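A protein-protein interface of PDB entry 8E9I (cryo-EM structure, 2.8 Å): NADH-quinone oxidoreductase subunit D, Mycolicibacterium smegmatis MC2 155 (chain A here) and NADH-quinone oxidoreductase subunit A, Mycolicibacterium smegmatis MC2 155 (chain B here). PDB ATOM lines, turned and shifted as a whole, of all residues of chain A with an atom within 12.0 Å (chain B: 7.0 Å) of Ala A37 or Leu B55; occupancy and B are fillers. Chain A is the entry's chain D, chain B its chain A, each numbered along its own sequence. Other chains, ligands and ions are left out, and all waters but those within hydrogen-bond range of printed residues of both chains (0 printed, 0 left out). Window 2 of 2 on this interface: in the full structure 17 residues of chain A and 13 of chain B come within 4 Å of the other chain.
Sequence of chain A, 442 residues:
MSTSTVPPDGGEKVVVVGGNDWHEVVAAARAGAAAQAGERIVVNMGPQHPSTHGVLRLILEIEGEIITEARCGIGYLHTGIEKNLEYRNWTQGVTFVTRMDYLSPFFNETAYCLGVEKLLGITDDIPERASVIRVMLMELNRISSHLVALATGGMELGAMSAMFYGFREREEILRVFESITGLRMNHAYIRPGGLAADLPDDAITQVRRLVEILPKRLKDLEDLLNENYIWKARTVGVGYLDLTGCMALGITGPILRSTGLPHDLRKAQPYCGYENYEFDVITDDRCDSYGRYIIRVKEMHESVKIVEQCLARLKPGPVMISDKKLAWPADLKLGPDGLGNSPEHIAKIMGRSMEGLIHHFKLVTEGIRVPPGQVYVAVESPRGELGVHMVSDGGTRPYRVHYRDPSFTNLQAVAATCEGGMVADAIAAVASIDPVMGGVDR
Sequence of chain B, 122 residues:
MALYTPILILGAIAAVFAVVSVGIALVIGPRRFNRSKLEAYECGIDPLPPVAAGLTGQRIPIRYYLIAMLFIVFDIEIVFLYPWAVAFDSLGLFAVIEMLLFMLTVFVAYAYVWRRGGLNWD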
ATOM      1  N   GLN A  36     -13.790  12.894 -21.002  1.00  0.00           N
ATOM      2  CA  GLN A  36     -15.030  13.631 -21.206  1.00  0.00           C
ATOM      3  C   GLN A  36     -15.699  13.927 -19.868  1.00  0.00           C
ATOM      4  O   GLN A  36     -15.035  13.983 -18.835  1.00  0.00           O
ATOM      5  CB  GLN A  36     -15.979  12.843 -22.111  1.00  0.00           C
ATOM      6  N   ALA A  37     -17.015  14.132 -19.894  1.00  0.00           N
ATOM      7  CA  ALA A  37     -17.768  14.264 -18.656  1.00  0.00           C
ATOM      8  C   ALA A  37     -17.839  12.918 -17.946  1.00  0.00           C
ATOM      9  O   ALA A  37     -17.909  11.859 -18.576  1.00  0.00           O
ATOM     10  CB  ALA A  37     -19.175  14.787 -18.932  1.00  0.00           C
ATOM     11  N   GLY A  38     -17.836  12.968 -16.616  1.00  0.00           N
ATOM     12  CA  GLY A  38     -17.663  11.804 -15.787  1.00  0.00           C
ATOM     13  C   GLY A  38     -16.370  11.823 -15.000  1.00  0.00           C
ATOM     14  O   GLY A  38     -16.288  11.199 -13.938  1.00  0.00           O
ATOM     15  N   GLU A  39     -15.365  12.545 -15.495  1.00  0.00           N
ATOM     16  CA  GLU A  39     -14.100  12.715 -14.802  1.00  0.00           C
ATOM     17  C   GLU A  39     -13.885  14.131 -14.286  1.00  0.00           C
ATOM     18  O   GLU A  39     -12.897  14.370 -13.585  1.00  0.00           O
ATOM     19  CB  GLU A  39     -12.937  12.338 -15.730  1.00  0.00           C
ATOM     20  N   ARG A  40     -14.771  15.068 -14.613  1.00  0.00           N
ATOM     21  CA  ARG A  40     -14.673  16.445 -14.148  1.00  0.00           C
ATOM     22  C   ARG A  40     -15.844  16.748 -13.225  1.00  0.00           C
ATOM     23  O   ARG A  40     -16.996  16.456 -13.558  1.00  0.00           O
ATOM     24  CB  ARG A  40     -14.668  17.425 -15.320  1.00  0.00           C
ATOM     25  CG  ARG A  40     -13.445  17.357 -16.213  1.00  0.00           C
ATOM     26  CD  ARG A  40     -13.470  18.496 -17.221  1.00  0.00           C
ATOM     27  NE  ARG A  40     -12.602  18.264 -18.368  1.00  0.00           N
ATOM     28  CZ  ARG A  40     -11.283  18.399 -18.354  1.00  0.00           C
ATOM     29  NH1 ARG A  40     -10.637  18.758 -17.259  1.00  0.00           N
ATOM     30  NH2 ARG A  40     -10.596  18.170 -19.467  1.00  0.00           N
ATOM     31  N   ILE A  41     -15.543  17.333 -12.069  1.00  0.00           N
ATOM     32  CA  ILE A  41     -16.576  17.818 -11.165  1.00  0.00           C
ATOM     33  C   ILE A  41     -16.782  19.312 -11.391  1.00  0.00           C
ATOM     34  O   ILE A  41     -15.903  20.021 -11.874  1.00  0.00           O
ATOM     35  CB  ILE A  41     -16.204  17.529  -9.701  1.00  0.00           C
ATOM     36  CG1 ILE A  41     -15.783  16.070  -9.539  1.00  0.00           C
ATOM     37  CG2 ILE A  41     -17.357  17.866  -8.777  1.00  0.00           C
ATOM     38  CD1 ILE A  41     -14.289  15.856  -9.652  1.00  0.00           C
ATOM     39  N   VAL A  42     -17.969  19.792 -11.043  1.00  0.00           N
ATOM     40  CA  VAL A  42     -18.266  21.219 -11.053  1.00  0.00           C
ATOM     41  C   VAL A  42     -18.614  21.631  -9.632  1.00  0.00           C
ATOM     42  O   VAL A  42     -19.559  21.102  -9.039  1.00  0.00           O
ATOM     43  CB  VAL A  42     -19.407  21.568 -12.025  1.00  0.00           C
ATOM     44  CG1 VAL A  42     -20.639  20.734 -11.737  1.00  0.00           C
ATOM     45  CG2 VAL A  42     -19.727  23.043 -11.941  1.00  0.00           C
ATOM     46  N   GLU A  61     -14.777  24.059 -12.857  1.00  0.00           N
ATOM     47  CA  GLU A  61     -14.774  22.717 -13.418  1.00  0.00           C
ATOM     48  C   GLU A  61     -13.390  22.120 -13.228  1.00  0.00           C
ATOM     49  O   GLU A  61     -12.414  22.592 -13.816  1.00  0.00           O
ATOM     50  CB  GLU A  61     -15.144  22.751 -14.897  1.00  0.00           C
ATOM     51  N   ILE A  62     -13.302  21.087 -12.397  1.00  0.00           N
ATOM     52  CA  ILE A  62     -12.030  20.566 -11.918  1.00  0.00           C
ATOM     53  C   ILE A  62     -11.905  19.107 -12.325  1.00  0.00           C
ATOM     54  O   ILE A  62     -12.820  18.312 -12.090  1.00  0.00           O
ATOM     55  CB  ILE A  62     -11.901  20.726 -10.391  1.00  0.00           C
ATOM     56  CG1 ILE A  62     -12.950  19.889  -9.661  1.00  0.00           C
ATOM     57  CG2 ILE A  62     -12.059  22.182 -10.013  1.00  0.00           C
ATOM     58  CD1 ILE A  62     -12.960  20.098  -8.169  1.00  0.00           C
ATOM     59  N   GLU A  63     -10.780  18.762 -12.945  1.00  0.00           N
ATOM     60  CA  GLU A  63     -10.467  17.382 -13.313  1.00  0.00           C
ATOM     61  C   GLU A  63      -9.703  16.781 -12.140  1.00  0.00           C
ATOM     62  O   GLU A  63      -8.473  16.786 -12.101  1.00  0.00           O
ATOM     63  CB  GLU A  63      -9.663  17.320 -14.607  1.00  0.00           C
ATOM     64  N   GLY A  64     -10.448  16.268 -11.172  1.00  0.00           N
ATOM     65  CA  GLY A  64      -9.854  15.745  -9.963  1.00  0.00           C
ATOM     66  C   GLY A  64      -9.536  16.860  -8.995  1.00  0.00           C
ATOM     67  O   GLY A  64     -10.277  17.072  -8.031  1.00  0.00           O
ATOM     68  N   THR A  68     -10.033  23.255 -14.561  1.00  0.00           N
ATOM     69  CA  THR A  68     -10.172  23.196 -16.010  1.00  0.00           C
ATOM     70  C   THR A  68     -10.807  24.471 -16.560  1.00  0.00           C
ATOM     71  O   THR A  68     -10.341  25.017 -17.562  1.00  0.00           O
ATOM     72  CB  THR A  68     -10.998  21.974 -16.410  1.00  0.00           C
ATOM     73  OG1 THR A  68     -10.528  20.829 -15.694  1.00  0.00           O
ATOM     74  CG2 THR A  68     -10.865  21.706 -17.896  1.00  0.00           C
ATOM     75  N   ARG A  71     -15.406  29.803 -14.121  1.00  0.00           N
ATOM     76  CA  ARG A  71     -16.432  30.816 -14.292  1.00  0.00           C
ATOM     77  C   ARG A  71     -16.514  31.676 -13.040  1.00  0.00           C
ATOM     78  O   ARG A  71     -16.257  31.216 -11.928  1.00  0.00           O
ATOM     79  CB  ARG A  71     -17.779  30.164 -14.578  1.00  0.00           C
ATOM     80  CG  ARG A  71     -17.888  29.610 -15.975  1.00  0.00           C
ATOM     81  CD  ARG A  71     -19.213  28.935 -16.208  1.00  0.00           C
ATOM     82  NE  ARG A  71     -19.330  28.492 -17.590  1.00  0.00           N
ATOM     83  CZ  ARG A  71     -18.752  27.402 -18.076  1.00  0.00           C
ATOM     84  NH1 ARG A  71     -18.041  26.595 -17.307  1.00  0.00           N
ATOM     85  NH2 ARG A  71     -18.888  27.117 -19.367  1.00  0.00           N
ATOM     86  N   ALA B  52     -26.912  13.942 -10.183  1.00  0.00           N
ATOM     87  CA  ALA B  52     -25.900  14.993 -10.170  1.00  0.00           C
ATOM     88  C   ALA B  52     -25.708  15.585 -11.554  1.00  0.00           C
ATOM     89  O   ALA B  52     -25.763  16.806 -11.734  1.00  0.00           O
ATOM     90  CB  ALA B  52     -24.571  14.444  -9.647  1.00  0.00           C
ATOM     91  N   ALA B  53     -25.495  14.720 -12.537  1.00  0.00           N
ATOM     92  CA  ALA B  53     -25.425  15.141 -13.926  1.00  0.00           C
ATOM     93  C   ALA B  53     -25.205  13.922 -14.806  1.00  0.00           C
ATOM     94  O   ALA B  53     -24.876  12.842 -14.303  1.00  0.00           O
ATOM     95  CB  ALA B  53     -24.309  16.168 -14.122  1.00  0.00           C
ATOM     96  N   GLY B  54     -25.398  14.072 -16.113  1.00  0.00           N
ATOM     97  CA  GLY B  54     -24.945  13.053 -17.032  1.00  0.00           C
ATOM     98  C   GLY B  54     -23.459  12.848 -16.828  1.00  0.00           C
ATOM     99  O   GLY B  54     -22.668  13.770 -17.049  1.00  0.00           O
ATOM    100  N   LEU B  55     -23.068  11.652 -16.395  1.00  0.00           N
ATOM    101  CA  LEU B  55     -21.692  11.410 -15.983  1.00  0.00           C
ATOM    102  C   LEU B  55     -21.425  12.164 -14.686  1.00  0.00           C
ATOM    103  O   LEU B  55     -21.894  11.748 -13.622  1.00  0.00           O
ATOM    104  CB  LEU B  55     -20.713  11.822 -17.086  1.00  0.00           C
ATOM    105  N   THR B  56     -20.682  13.268 -14.758  1.00  0.00           N
ATOM    106  CA  THR B  56     -20.415  14.094 -13.585  1.00  0.00           C
ATOM    107  C   THR B  56     -19.398  13.437 -12.663  1.00  0.00           C
ATOM    108  O   THR B  56     -18.652  12.550 -13.084  1.00  0.00           O
ATOM    109  CB  THR B  56     -21.708  14.372 -12.816  1.00  0.00           C
ATOM    110  N   GLY B  57     -19.372  13.845 -11.398  1.00  0.00           N
ATOM    111  CA  GLY B  57     -18.313  13.431 -10.501  1.00  0.00           C
ATOM    112  C   GLY B  57     -18.411  11.989 -10.054  1.00  0.00           C
ATOM    113  O   GLY B  57     -18.351  11.695  -8.857  1.00  0.00           O
ATOM    114  N   GLN B  58     -18.558  11.073 -11.007  1.00  0.00           N
ATOM    115  CA  GLN B  58     -18.512   9.660 -10.677  1.00  0.00           C
ATOM    116  C   GLN B  58     -17.095   9.179 -10.418  1.00  0.00           C
ATOM    117  O   GLN B  58     -16.899   8.302  -9.576  1.00  0.00           O
ATOM    118  CB  GLN B  58     -19.126   8.833 -11.806  1.00  0.00           C
ATOM    119  CG  GLN B  58     -20.531   9.233 -12.171  1.00  0.00           C
ATOM    120  CD  GLN B  58     -21.196   8.223 -13.076  1.00  0.00           C
ATOM    121  OE1 GLN B  58     -20.734   7.092 -13.199  1.00  0.00           O
ATOM    122  NE2 GLN B  58     -22.289   8.624 -13.712  1.00  0.00           N
ATOM    123  N   ARG B  59     -16.107   9.743 -11.107  1.00  0.00           N
ATOM    124  CA  ARG B  59     -14.736   9.254 -11.054  1.00  0.00           C
ATOM    125  C   ARG B  59     -13.799  10.428 -10.850  1.00  0.00           C
ATOM    126  O   ARG B  59     -13.859  11.407 -11.597  1.00  0.00           O
ATOM    127  CB  ARG B  59     -14.396   8.500 -12.338  1.00  0.00           C
ATOM    128  CG  ARG B  59     -15.013   7.111 -12.396  1.00  0.00           C
ATOM    129  CD  ARG B  59     -14.745   6.411 -13.709  1.00  0.00           C
ATOM    130  NE  ARG B  59     -15.365   7.108 -14.827  1.00  0.00           N
ATOM    131  CZ  ARG B  59     -14.788   8.070 -15.532  1.00  0.00           C
ATOM    132  NH1 ARG B  59     -13.564   8.493 -15.257  1.00  0.00           N
ATOM    133  NH2 ARG B  59     -15.457   8.623 -16.538  1.00  0.00           N
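N of Arg B59 is in hydrogen-bond range of O of Gly A38, at 3.2 Å.
O of Gly A38 lies close to O of Thr B56 (2.9 Å).
O of Leu B55 is in hydrogen-bond range of NE2 of Gln B58 (3.2 Å).
NH1 of Arg A40 is in hydrogen-bond range of OG1 of Thr A68 (2.6 Å).
The backbone carbonyl oxygen (O) of Ile A41 sits at hydrogen-bond distance from the backbone NH (N) of Ile A62, at 2.9 Å.
Among the printed residues, pairs that only touch across the chains: Ala A37 with Leu B55 (3.2 Å), Gly A38 with Leu B55 (3.1 Å), Gly A38 with Gln B58 (3.7 Å), Glu A39 with Arg B59 (3.5 Å), Arg A40 with Thr B56 (3.96 Å) and Ile A41 with Gly B57 (3.8 Å).
Ala A37 touches just one residue of chain B: Leu B55 (3.2 Å).
Leu B55 touches just these residues of chain A: Ala A37 and Gly A38.
No residue of chain A comes within 4 Å of Ala B52.
No residue of chain A comes within 4 Å of Ala B53.
Gly B54 touches none of the printed residues of chain A.
Of chain A, only Gly A38 and Arg A40 come within 4 Å of Thr B56.
Of the printed residues of chain A, Gln B58 touches Gly A38 (3.7 Å).
Printed residues of chain B within 4 Å of Glu A39: Arg B59 (3.5 Å).
Printed residues of chain B within 4 Å of Gly A38: Leu B55 (3.1 Å), Thr B56 (2.9 Å), Gln B58 (3.7 Å) and Arg B59 (3.2 Å).
Of the printed residues of chain B, Ile A41 touches Gly B57.
Of the printed residues of chain B, Arg A40 touches Thr B56 (3.96 Å).
Printed residues of chain A within 4 Å of Arg B59: Gly A38 (3.2 Å) and Glu A39 (3.5 Å).
The nearest residue of chain B that does not touch Ala A37 is Gly B54 (4.1 Å).
The nearest printed residue of chain A that does not touch Arg B59 is Ala A37 (4.5 Å).
Of the 8 printed residues of chain B, 5 touch a printed residue of chain A.
Printed residues of chain B that touch a printed residue of chain A: Leu B55, Thr B56, Gly B57, Gln B58 and Arg B59.
Hydrophobic or aromatic side chains of chain B within 4 Å of the printed part of chain A: Leu B55.
Hydrophobic or aromatic side chains of chain A that line the printed part of chain B: Ala A37 and Ile A41.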
